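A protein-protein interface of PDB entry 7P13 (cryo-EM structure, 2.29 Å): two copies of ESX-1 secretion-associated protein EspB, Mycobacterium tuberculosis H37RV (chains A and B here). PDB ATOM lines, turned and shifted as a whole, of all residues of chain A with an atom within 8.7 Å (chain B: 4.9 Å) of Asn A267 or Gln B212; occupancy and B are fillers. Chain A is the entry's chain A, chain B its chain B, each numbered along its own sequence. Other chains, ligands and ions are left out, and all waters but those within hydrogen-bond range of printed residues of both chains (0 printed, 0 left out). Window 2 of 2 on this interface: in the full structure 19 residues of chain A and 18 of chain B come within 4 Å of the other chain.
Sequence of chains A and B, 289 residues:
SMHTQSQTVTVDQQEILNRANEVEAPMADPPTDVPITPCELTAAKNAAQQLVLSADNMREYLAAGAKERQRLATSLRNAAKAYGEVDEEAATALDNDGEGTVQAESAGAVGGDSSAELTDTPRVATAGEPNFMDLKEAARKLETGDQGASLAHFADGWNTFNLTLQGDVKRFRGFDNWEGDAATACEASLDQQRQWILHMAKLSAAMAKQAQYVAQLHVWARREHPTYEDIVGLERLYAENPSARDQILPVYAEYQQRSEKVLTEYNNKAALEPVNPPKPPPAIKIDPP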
ATOM      1  N   LEU A  41       0.131  13.623 -25.852  1.00  0.00           N
ATOM      2  CA  LEU A  41      -0.238  12.253 -25.561  1.00  0.00           C
ATOM      3  C   LEU A  41       0.995  11.379 -25.434  1.00  0.00           C
ATOM      4  O   LEU A  41       2.007  11.599 -26.093  1.00  0.00           O
ATOM      5  CB  LEU A  41      -1.134  11.714 -26.650  1.00  0.00           C
ATOM      6  CG  LEU A  41      -2.509  12.348 -26.538  1.00  0.00           C
ATOM      7  CD1 LEU A  41      -3.407  11.853 -27.635  1.00  0.00           C
ATOM      8  CD2 LEU A  41      -3.092  12.050 -25.172  1.00  0.00           C
ATOM      9  N   THR A  42       0.905  10.392 -24.555  1.00  0.00           N
ATOM     10  CA  THR A  42       2.009   9.469 -24.376  1.00  0.00           C
ATOM     11  C   THR A  42       2.298   8.676 -25.640  1.00  0.00           C
ATOM     12  O   THR A  42       3.463   8.435 -25.964  1.00  0.00           O
ATOM     13  CB  THR A  42       1.726   8.533 -23.217  1.00  0.00           C
ATOM     14  OG1 THR A  42       1.723   9.287 -22.012  1.00  0.00           O
ATOM     15  CG2 THR A  42       2.774   7.490 -23.139  1.00  0.00           C
ATOM     16  N   ALA A  43       1.259   8.263 -26.362  1.00  0.00           N
ATOM     17  CA  ALA A  43       1.477   7.529 -27.601  1.00  0.00           C
ATOM     18  C   ALA A  43       2.199   8.384 -28.627  1.00  0.00           C
ATOM     19  O   ALA A  43       3.085   7.901 -29.334  1.00  0.00           O
ATOM     20  CB  ALA A  43       0.156   7.028 -28.163  1.00  0.00           C
ATOM     21  N   ALA A  44       1.862   9.666 -28.691  1.00  0.00           N
ATOM     22  CA  ALA A  44       2.533  10.550 -29.628  1.00  0.00           C
ATOM     23  C   ALA A  44       3.999  10.735 -29.268  1.00  0.00           C
ATOM     24  O   ALA A  44       4.868  10.698 -30.142  1.00  0.00           O
ATOM     25  CB  ALA A  44       1.807  11.892 -29.683  1.00  0.00           C
ATOM     26  N   ASN A  46       5.872   8.686 -27.551  1.00  0.00           N
ATOM     27  CA  ASN A  46       6.576   7.440 -27.784  1.00  0.00           C
ATOM     28  C   ASN A  46       6.839   7.229 -29.266  1.00  0.00           C
ATOM     29  O   ASN A  46       7.900   6.734 -29.641  1.00  0.00           O
ATOM     30  CB  ASN A  46       5.797   6.286 -27.186  1.00  0.00           C
ATOM     31  CG  ASN A  46       5.930   6.222 -25.696  1.00  0.00           C
ATOM     32  OD1 ASN A  46       6.677   6.979 -25.096  1.00  0.00           O
ATOM     33  ND2 ASN A  46       5.205   5.318 -25.084  1.00  0.00           N
ATOM     34  N   ALA A  47       5.900   7.619 -30.120  1.00  0.00           N
ATOM     35  CA  ALA A  47       6.133   7.534 -31.554  1.00  0.00           C
ATOM     36  C   ALA A  47       7.275   8.438 -31.986  1.00  0.00           C
ATOM     37  O   ALA A  47       8.107   8.047 -32.811  1.00  0.00           O
ATOM     38  CB  ALA A  47       4.862   7.887 -32.311  1.00  0.00           C
ATOM     39  N   LEU A 217      -2.332  10.477 -38.563  1.00  0.00           N
ATOM     40  CA  LEU A 217      -3.087  10.022 -37.413  1.00  0.00           C
ATOM     41  C   LEU A 217      -3.405  11.167 -36.472  1.00  0.00           C
ATOM     42  O   LEU A 217      -4.517  11.260 -35.957  1.00  0.00           O
ATOM     43  CB  LEU A 217      -2.311   8.942 -36.677  1.00  0.00           C
ATOM     44  CG  LEU A 217      -3.064   8.456 -35.442  1.00  0.00           C
ATOM     45  CD1 LEU A 217      -4.240   7.615 -35.868  1.00  0.00           C
ATOM     46  CD2 LEU A 217      -2.166   7.683 -34.494  1.00  0.00           C
ATOM     47  N   TRP A 220      -6.215  13.255 -37.972  1.00  0.00           N
ATOM     48  CA  TRP A 220      -7.499  12.606 -37.758  1.00  0.00           C
ATOM     49  C   TRP A 220      -7.943  12.750 -36.309  1.00  0.00           C
ATOM     50  O   TRP A 220      -9.122  12.969 -36.028  1.00  0.00           O
ATOM     51  CB  TRP A 220      -7.410  11.139 -38.164  1.00  0.00           C
ATOM     52  CG  TRP A 220      -8.609  10.353 -37.839  1.00  0.00           C
ATOM     53  CD1 TRP A 220      -9.687  10.175 -38.613  1.00  0.00           C
ATOM     54  CD2 TRP A 220      -8.856   9.631 -36.638  1.00  0.00           C
ATOM     55  NE1 TRP A 220     -10.602   9.399 -37.983  1.00  0.00           N
ATOM     56  CE2 TRP A 220     -10.117   9.057 -36.756  1.00  0.00           C
ATOM     57  CE3 TRP A 220      -8.139   9.443 -35.459  1.00  0.00           C
ATOM     58  CZ2 TRP A 220     -10.667   8.279 -35.764  1.00  0.00           C
ATOM     59  CZ3 TRP A 220      -8.685   8.684 -34.476  1.00  0.00           C
ATOM     60  CH2 TRP A 220      -9.938   8.110 -34.627  1.00  0.00           C
ATOM     61  N   ALA A 221      -7.009  12.642 -35.381  1.00  0.00           N
ATOM     62  CA  ALA A 221      -7.352  12.756 -33.977  1.00  0.00           C
ATOM     63  C   ALA A 221      -7.855  14.147 -33.637  1.00  0.00           C
ATOM     64  O   ALA A 221      -8.793  14.292 -32.857  1.00  0.00           O
ATOM     65  CB  ALA A 221      -6.147  12.401 -33.125  1.00  0.00           C
ATOM     66  N   GLU A 260     -13.037   8.716 -25.900  1.00  0.00           N
ATOM     67  CA  GLU A 260     -12.518   7.399 -25.671  1.00  0.00           C
ATOM     68  C   GLU A 260     -12.204   6.711 -26.969  1.00  0.00           C
ATOM     69  O   GLU A 260     -11.250   5.945 -27.050  1.00  0.00           O
ATOM     70  CB  GLU A 260     -13.524   6.628 -24.856  1.00  0.00           C
ATOM     71  CG  GLU A 260     -13.089   5.319 -24.273  1.00  0.00           C
ATOM     72  CD  GLU A 260     -13.182   4.129 -25.220  1.00  0.00           C
ATOM     73  OE1 GLU A 260     -13.855   4.221 -26.264  1.00  0.00           O
ATOM     74  OE2 GLU A 260     -12.570   3.086 -24.909  1.00  0.00           O
ATOM     75  N   LYS A 261     -12.972   6.984 -27.999  1.00  0.00           N
ATOM     76  CA  LYS A 261     -12.642   6.298 -29.213  1.00  0.00           C
ATOM     77  C   LYS A 261     -11.436   6.918 -29.881  1.00  0.00           C
ATOM     78  O   LYS A 261     -10.736   6.231 -30.618  1.00  0.00           O
ATOM     79  CB  LYS A 261     -13.823   6.291 -30.151  1.00  0.00           C
ATOM     80  CG  LYS A 261     -13.652   5.314 -31.226  1.00  0.00           C
ATOM     81  CD  LYS A 261     -14.700   5.495 -32.233  1.00  0.00           C
ATOM     82  CE  LYS A 261     -14.824   6.953 -32.564  1.00  0.00           C
ATOM     83  NZ  LYS A 261     -13.576   7.503 -33.075  1.00  0.00           N
ATOM     84  N   VAL A 262     -11.155   8.180 -29.608  1.00  0.00           N
ATOM     85  CA  VAL A 262     -10.036   8.796 -30.286  1.00  0.00           C
ATOM     86  C   VAL A 262      -8.736   8.383 -29.634  1.00  0.00           C
ATOM     87  O   VAL A 262      -7.844   7.859 -30.305  1.00  0.00           O
ATOM     88  CB  VAL A 262     -10.212  10.325 -30.328  1.00  0.00           C
ATOM     89  CG1 VAL A 262      -8.936  10.995 -30.722  1.00  0.00           C
ATOM     90  CG2 VAL A 262     -11.278  10.663 -31.338  1.00  0.00           C
ATOM     91  N   LEU A 263      -8.648   8.576 -28.317  1.00  0.00           N
ATOM     92  CA  LEU A 263      -7.434   8.296 -27.563  1.00  0.00           C
ATOM     93  C   LEU A 263      -7.006   6.855 -27.729  1.00  0.00           C
ATOM     94  O   LEU A 263      -5.842   6.572 -28.026  1.00  0.00           O
ATOM     95  CB  LEU A 263      -7.661   8.600 -26.093  1.00  0.00           C
ATOM     96  CG  LEU A 263      -7.857  10.058 -25.734  1.00  0.00           C
ATOM     97  CD1 LEU A 263      -7.731  10.218 -24.261  1.00  0.00           C
ATOM     98  CD2 LEU A 263      -6.856  10.931 -26.442  1.00  0.00           C
ATOM     99  N   THR A 264      -7.966   5.948 -27.645  1.00  0.00           N
ATOM    100  CA  THR A 264      -7.684   4.539 -27.828  1.00  0.00           C
ATOM    101  C   THR A 264      -7.170   4.265 -29.221  1.00  0.00           C
ATOM    102  O   THR A 264      -6.156   3.579 -29.389  1.00  0.00           O
ATOM    103  CB  THR A 264      -8.942   3.738 -27.538  1.00  0.00           C
ATOM    104  OG1 THR A 264      -9.175   3.720 -26.139  1.00  0.00           O
ATOM    105  CG2 THR A 264      -8.863   2.366 -27.986  1.00  0.00           C
ATOM    106  N   GLU A 265      -7.822   4.851 -30.217  1.00  0.00           N
ATOM    107  CA  GLU A 265      -7.361   4.699 -31.579  1.00  0.00           C
ATOM    108  C   GLU A 265      -5.972   5.283 -31.732  1.00  0.00           C
ATOM    109  O   GLU A 265      -5.081   4.624 -32.278  1.00  0.00           O
ATOM    110  CB  GLU A 265      -8.355   5.350 -32.528  1.00  0.00           C
ATOM    111  CG  GLU A 265      -8.007   5.234 -33.970  1.00  0.00           C
ATOM    112  CD  GLU A 265      -8.204   3.849 -34.506  1.00  0.00           C
ATOM    113  OE1 GLU A 265      -8.447   2.926 -33.717  1.00  0.00           O
ATOM    114  OE2 GLU A 265      -8.134   3.681 -35.735  1.00  0.00           O
ATOM    115  N   TYR A 266      -5.734   6.430 -31.093  1.00  0.00           N
ATOM    116  CA  TYR A 266      -4.435   7.070 -31.153  1.00  0.00           C
ATOM    117  C   TYR A 266      -3.383   6.186 -30.531  1.00  0.00           C
ATOM    118  O   TYR A 266      -2.258   6.116 -31.016  1.00  0.00           O
ATOM    119  CB  TYR A 266      -4.453   8.377 -30.388  1.00  0.00           C
ATOM    120  CG  TYR A 266      -3.465   9.403 -30.839  1.00  0.00           C
ATOM    121  CD1 TYR A 266      -3.859  10.431 -31.650  1.00  0.00           C
ATOM    122  CD2 TYR A 266      -2.116   9.284 -30.553  1.00  0.00           C
ATOM    123  CE1 TYR A 266      -2.985  11.388 -32.070  1.00  0.00           C
ATOM    124  CE2 TYR A 266      -1.214  10.217 -31.002  1.00  0.00           C
ATOM    125  CZ  TYR A 266      -1.664  11.277 -31.759  1.00  0.00           C
ATOM    126  OH  TYR A 266      -0.807  12.226 -32.213  1.00  0.00           O
ATOM    127  N   ASN A 267      -3.759   5.450 -29.505  1.00  0.00           N
ATOM    128  CA  ASN A 267      -2.785   4.652 -28.808  1.00  0.00           C
ATOM    129  C   ASN A 267      -2.407   3.420 -29.591  1.00  0.00           C
ATOM    130  O   ASN A 267      -1.269   2.966 -29.502  1.00  0.00           O
ATOM    131  CB  ASN A 267      -3.342   4.302 -27.458  1.00  0.00           C
ATOM    132  CG  ASN A 267      -2.347   3.842 -26.511  1.00  0.00           C
ATOM    133  OD1 ASN A 267      -1.231   3.492 -26.849  1.00  0.00           O
ATOM    134  ND2 ASN A 267      -2.710   3.933 -25.260  1.00  0.00           N
ATOM    135  N   ASN A 268      -3.325   2.893 -30.371  1.00  0.00           N
ATOM    136  CA  ASN A 268      -3.078   1.665 -31.082  1.00  0.00           C
ATOM    137  C   ASN A 268      -2.435   1.878 -32.427  1.00  0.00           C
ATOM    138  O   ASN A 268      -1.558   1.111 -32.805  1.00  0.00           O
ATOM    139  CB  ASN A 268      -4.373   0.905 -31.200  1.00  0.00           C
ATOM    140  CG  ASN A 268      -4.909   0.488 -29.870  1.00  0.00           C
ATOM    141  OD1 ASN A 268      -4.208   0.484 -28.877  1.00  0.00           O
ATOM    142  ND2 ASN A 268      -6.149   0.147 -29.835  1.00  0.00           N
ATOM    143  N   LYS A 269      -2.817   2.905 -33.156  1.00  0.00           N
ATOM    144  CA  LYS A 269      -2.205   3.089 -34.453  1.00  0.00           C
ATOM    145  C   LYS A 269      -0.846   3.731 -34.356  1.00  0.00           C
ATOM    146  O   LYS A 269      -0.097   3.684 -35.322  1.00  0.00           O
ATOM    147  CB  LYS A 269      -3.082   3.940 -35.348  1.00  0.00           C
ATOM    148  CG  LYS A 269      -4.468   3.513 -35.389  1.00  0.00           C
ATOM    149  CD  LYS A 269      -4.556   2.158 -35.886  1.00  0.00           C
ATOM    150  CE  LYS A 269      -5.785   2.029 -36.696  1.00  0.00           C
ATOM    151  NZ  LYS A 269      -5.945   0.631 -37.122  1.00  0.00           N
ATOM    152  N   ALA A 270      -0.510   4.312 -33.224  1.00  0.00           N
ATOM    153  CA  ALA A 270       0.711   5.081 -33.116  1.00  0.00           C
ATOM    154  C   ALA A 270       1.918   4.254 -32.716  1.00  0.00           C
ATOM    155  O   ALA A 270       3.031   4.776 -32.739  1.00  0.00           O
ATOM    156  CB  ALA A 270       0.534   6.215 -32.118  1.00  0.00           C
ATOM    157  N   ALA A 271       1.742   3.002 -32.350  1.00  0.00           N
ATOM    158  CA  ALA A 271       2.886   2.164 -32.041  1.00  0.00           C
ATOM    159  C   ALA A 271       3.613   1.801 -33.327  1.00  0.00           C
ATOM    160  O   ALA A 271       3.026   1.223 -34.238  1.00  0.00           O
ATOM    161  CB  ALA A 271       2.431   0.918 -31.303  1.00  0.00           C
ATOM    162  N   LEU A 272       4.888   2.140 -33.405  1.00  0.00           N
ATOM    163  CA  LEU A 272       5.655   2.023 -34.628  1.00  0.00           C
ATOM    164  C   LEU A 272       6.690   0.923 -34.518  1.00  0.00           C
ATOM    165  O   LEU A 272       7.286   0.730 -33.464  1.00  0.00           O
ATOM    166  CB  LEU A 272       6.359   3.325 -34.938  1.00  0.00           C
ATOM    167  CG  LEU A 272       5.406   4.431 -35.298  1.00  0.00           C
ATOM    168  CD1 LEU A 272       6.186   5.723 -35.363  1.00  0.00           C
ATOM    169  CD2 LEU A 272       4.765   4.123 -36.611  1.00  0.00           C
ATOM    170  N   ALA B 155       1.614  -0.839 -18.672  1.00  0.00           N
ATOM    171  CA  ALA B 155       1.901  -0.728 -20.091  1.00  0.00           C
ATOM    172  C   ALA B 155       2.810   0.452 -20.386  1.00  0.00           C
ATOM    173  O   ALA B 155       3.685   0.356 -21.247  1.00  0.00           O
ATOM    174  CB  ALA B 155       0.607  -0.613 -20.885  1.00  0.00           C
ATOM    175  N   ASP B 156       2.610   1.572 -19.691  1.00  0.00           N
ATOM    176  CA  ASP B 156       3.486   2.713 -19.897  1.00  0.00           C
ATOM    177  C   ASP B 156       4.913   2.386 -19.507  1.00  0.00           C
ATOM    178  O   ASP B 156       5.851   2.736 -20.228  1.00  0.00           O
ATOM    179  CB  ASP B 156       3.007   3.917 -19.105  1.00  0.00           C
ATOM    180  CG  ASP B 156       1.704   4.459 -19.602  1.00  0.00           C
ATOM    181  OD1 ASP B 156       1.503   4.555 -20.827  1.00  0.00           O
ATOM    182  OD2 ASP B 156       0.853   4.799 -18.755  1.00  0.00           O
ATOM    183  N   ASN B 159       6.400   0.086 -22.259  1.00  0.00           N
ATOM    184  CA  ASN B 159       6.677   0.824 -23.486  1.00  0.00           C
ATOM    185  C   ASN B 159       7.914   1.695 -23.331  1.00  0.00           C
ATOM    186  O   ASN B 159       8.757   1.783 -24.241  1.00  0.00           O
ATOM    187  CB  ASN B 159       5.475   1.677 -23.860  1.00  0.00           C
ATOM    188  CG  ASN B 159       4.478   0.937 -24.686  1.00  0.00           C
ATOM    189  OD1 ASN B 159       4.830   0.057 -25.450  1.00  0.00           O
ATOM    190  ND2 ASN B 159       3.220   1.283 -24.538  1.00  0.00           N
ATOM    191  N   ALA B 208       3.252  -4.837 -23.398  1.00  0.00           N
ATOM    192  CA  ALA B 208       2.539  -3.606 -23.093  1.00  0.00           C
ATOM    193  C   ALA B 208       1.260  -3.490 -23.906  1.00  0.00           C
ATOM    194  O   ALA B 208       0.231  -3.041 -23.392  1.00  0.00           O
ATOM    195  CB  ALA B 208       3.439  -2.403 -23.329  1.00  0.00           C
ATOM    196  N   LYS B 209       1.305  -3.901 -25.170  1.00  0.00           N
ATOM    197  CA  LYS B 209       0.103  -3.902 -25.986  1.00  0.00           C
ATOM    198  C   LYS B 209      -0.948  -4.839 -25.420  1.00  0.00           C
ATOM    199  O   LYS B 209      -2.136  -4.538 -25.468  1.00  0.00           O
ATOM    200  CB  LYS B 209       0.423  -4.289 -27.420  1.00  0.00           C
ATOM    201  CG  LYS B 209       0.832  -3.165 -28.277  1.00  0.00           C
ATOM    202  CD  LYS B 209       1.036  -3.641 -29.680  1.00  0.00           C
ATOM    203  CE  LYS B 209       1.928  -2.711 -30.486  1.00  0.00           C
ATOM    204  NZ  LYS B 209       3.232  -2.414 -29.852  1.00  0.00           N
ATOM    205  N   GLN B 210      -0.529  -5.976 -24.888  1.00  0.00           N
ATOM    206  CA  GLN B 210      -1.483  -6.886 -24.273  1.00  0.00           C
ATOM    207  C   GLN B 210      -2.155  -6.266 -23.059  1.00  0.00           C
ATOM    208  O   GLN B 210      -3.369  -6.415 -22.868  1.00  0.00           O
ATOM    209  CB  GLN B 210      -0.793  -8.168 -23.881  1.00  0.00           C
ATOM    210  CG  GLN B 210      -0.747  -9.163 -24.950  1.00  0.00           C
ATOM    211  CD  GLN B 210       0.047 -10.334 -24.519  1.00  0.00           C
ATOM    212  OE1 GLN B 210       1.049 -10.175 -23.850  1.00  0.00           O
ATOM    213  NE2 GLN B 210      -0.407 -11.523 -24.853  1.00  0.00           N
ATOM    214  N   ALA B 211      -1.382  -5.584 -22.225  1.00  0.00           N
ATOM    215  CA  ALA B 211      -1.971  -4.906 -21.079  1.00  0.00           C
ATOM    216  C   ALA B 211      -2.958  -3.830 -21.512  1.00  0.00           C
ATOM    217  O   ALA B 211      -4.047  -3.710 -20.942  1.00  0.00           O
ATOM    218  CB  ALA B 211      -0.878  -4.308 -20.209  1.00  0.00           C
ATOM    219  N   GLN B 212      -2.606  -3.061 -22.533  1.00  0.00           N
ATOM    220  CA  GLN B 212      -3.525  -2.057 -23.033  1.00  0.00           C
ATOM    221  C   GLN B 212      -4.773  -2.678 -23.626  1.00  0.00           C
ATOM    222  O   GLN B 212      -5.858  -2.118 -23.497  1.00  0.00           O
ATOM    223  CB  GLN B 212      -2.839  -1.179 -24.061  1.00  0.00           C
ATOM    224  CG  GLN B 212      -1.954  -0.187 -23.425  1.00  0.00           C
ATOM    225  CD  GLN B 212      -1.204   0.632 -24.413  1.00  0.00           C
ATOM    226  OE1 GLN B 212      -1.179   0.318 -25.586  1.00  0.00           O
ATOM    227  NE2 GLN B 212      -0.587   1.692 -23.949  1.00  0.00           N
ATOM    228  N   TYR B 213      -4.641  -3.826 -24.265  1.00  0.00           N
ATOM    229  CA  TYR B 213      -5.792  -4.496 -24.840  1.00  0.00           C
ATOM    230  C   TYR B 213      -6.757  -4.959 -23.763  1.00  0.00           C
ATOM    231  O   TYR B 213      -7.973  -4.838 -23.919  1.00  0.00           O
ATOM    232  CB  TYR B 213      -5.317  -5.663 -25.681  1.00  0.00           C
ATOM    233  CG  TYR B 213      -6.403  -6.457 -26.316  1.00  0.00           C
ATOM    234  CD1 TYR B 213      -6.972  -6.049 -27.498  1.00  0.00           C
ATOM    235  CD2 TYR B 213      -6.857  -7.624 -25.742  1.00  0.00           C
ATOM    236  CE1 TYR B 213      -7.951  -6.771 -28.086  1.00  0.00           C
ATOM    237  CE2 TYR B 213      -7.837  -8.350 -26.317  1.00  0.00           C
ATOM    238  CZ  TYR B 213      -8.378  -7.929 -27.496  1.00  0.00           C
ATOM    239  OH  TYR B 213      -9.367  -8.664 -28.078  1.00  0.00           O
ATOM    240  N   VAL B 214      -6.232  -5.495 -22.669  1.00  0.00           N
ATOM    241  CA  VAL B 214      -7.102  -5.912 -21.583  1.00  0.00           C
ATOM    242  C   VAL B 214      -7.777  -4.707 -20.941  1.00  0.00           C
ATOM    243  O   VAL B 214      -8.951  -4.767 -20.570  1.00  0.00           O
ATOM    244  CB  VAL B 214      -6.315  -6.745 -20.558  1.00  0.00           C
ATOM    245  CG1 VAL B 214      -7.114  -6.924 -19.289  1.00  0.00           C
ATOM    246  CG2 VAL B 214      -5.985  -8.070 -21.137  1.00  0.00           C
ATOM    247  N   ALA B 215      -7.055  -3.600 -20.807  1.00  0.00           N
ATOM    248  CA  ALA B 215      -7.669  -2.397 -20.263  1.00  0.00           C
ATOM    249  C   ALA B 215      -8.787  -1.875 -21.160  1.00  0.00           C
ATOM    250  O   ALA B 215      -9.859  -1.498 -20.672  1.00  0.00           O
ATOM    251  CB  ALA B 215      -6.615  -1.322 -20.040  1.00  0.00           C
ATOM    252  N   GLN B 216      -8.567  -1.867 -22.471  1.00  0.00           N
ATOM    253  CA  GLN B 216      -9.610  -1.430 -23.387  1.00  0.00           C
ATOM    254  C   GLN B 216     -10.802  -2.366 -23.344  1.00  0.00           C
ATOM    255  O   GLN B 216     -11.948  -1.923 -23.443  1.00  0.00           O
ATOM    256  CB  GLN B 216      -9.069  -1.331 -24.802  1.00  0.00           C
ATOM    257  CG  GLN B 216      -8.190  -0.164 -25.006  1.00  0.00           C
ATOM    258  CD  GLN B 216      -7.231  -0.366 -26.138  1.00  0.00           C
ATOM    259  OE1 GLN B 216      -7.400  -1.261 -26.946  1.00  0.00           O
ATOM    260  NE2 GLN B 216      -6.215   0.458 -26.202  1.00  0.00           N
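NE2 of Gln B212 lies close to ND2 of Asn A267 (3.4 Å).
OD1 of Asn A268 is in hydrogen-bond range of NE2 of Gln B216, at 3.3 Å.
ND2 of Asn B159 lies close to O of Ala B155 (3.5 Å).
O of Thr A264 lies close to ND2 of Asn A268.
OG1 of Thr A264 lies within hydrogen-bond range of O of Glu A260 (3.2 Å).
Among the printed residues, pairs that only touch across the chains: Thr A42 with Asp B156 (3.9 Å), Asn A46 with Asn B159 (3.9 Å), Thr A264 with Gln B216 (3.7 Å) and Ala A271 with Lys B209 (3.7 Å).
Of chain B, only Gln B212 (3.4 Å) comes within 4 Å of Asn A267.
Of chain A, only Asn A267 (3.4 Å) comes within 4 Å of Gln B212.
Of the printed residues of chain B, Asn A46 touches Asn B159.
Of the printed residues of chain A, Asp B156 touches Thr A42 (3.9 Å).
Of the printed residues of chain A, Gln B216 touches Thr A264 (3.7 Å) and Asn A268 (3.3 Å).
Printed residues of chain B within 4 Å of Thr A42: Asp B156.
Of the printed residues of chain B, Asn A268 touches Gln B216.
The nearest printed residue of chain B that does not touch Asn A267 is Gln B216 (5.0 Å).
The nearest printed residue of chain B that does not touch Ala A271 is Asn B159 (6.4 Å).
Of the 12 printed residues of chain B, 5 touch a printed residue of chain A.
Printed residues of chain B that touch a printed residue of chain A: Asp B156, Asn B159, Lys B209, Gln B212 and Gln B216.
Along chain B the printed residues that touch a printed residue of chain A span positions 156 to 216.
Of the 22 printed residues of chain A, 6 touch a printed residue of chain B.
Hydrophobic or aromatic side chains of chain A that line the printed part of chain B: Ala A271.
Among the printed residues, no Asp or Glu carboxylate lies within 4 Å of a Lys or Arg side-chain nitrogen of the other chain.
No position is printed for both chains.
Of the 6 pairs that touch across the chains among the printed residues, none has its exchanged pair printed and touching as well.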
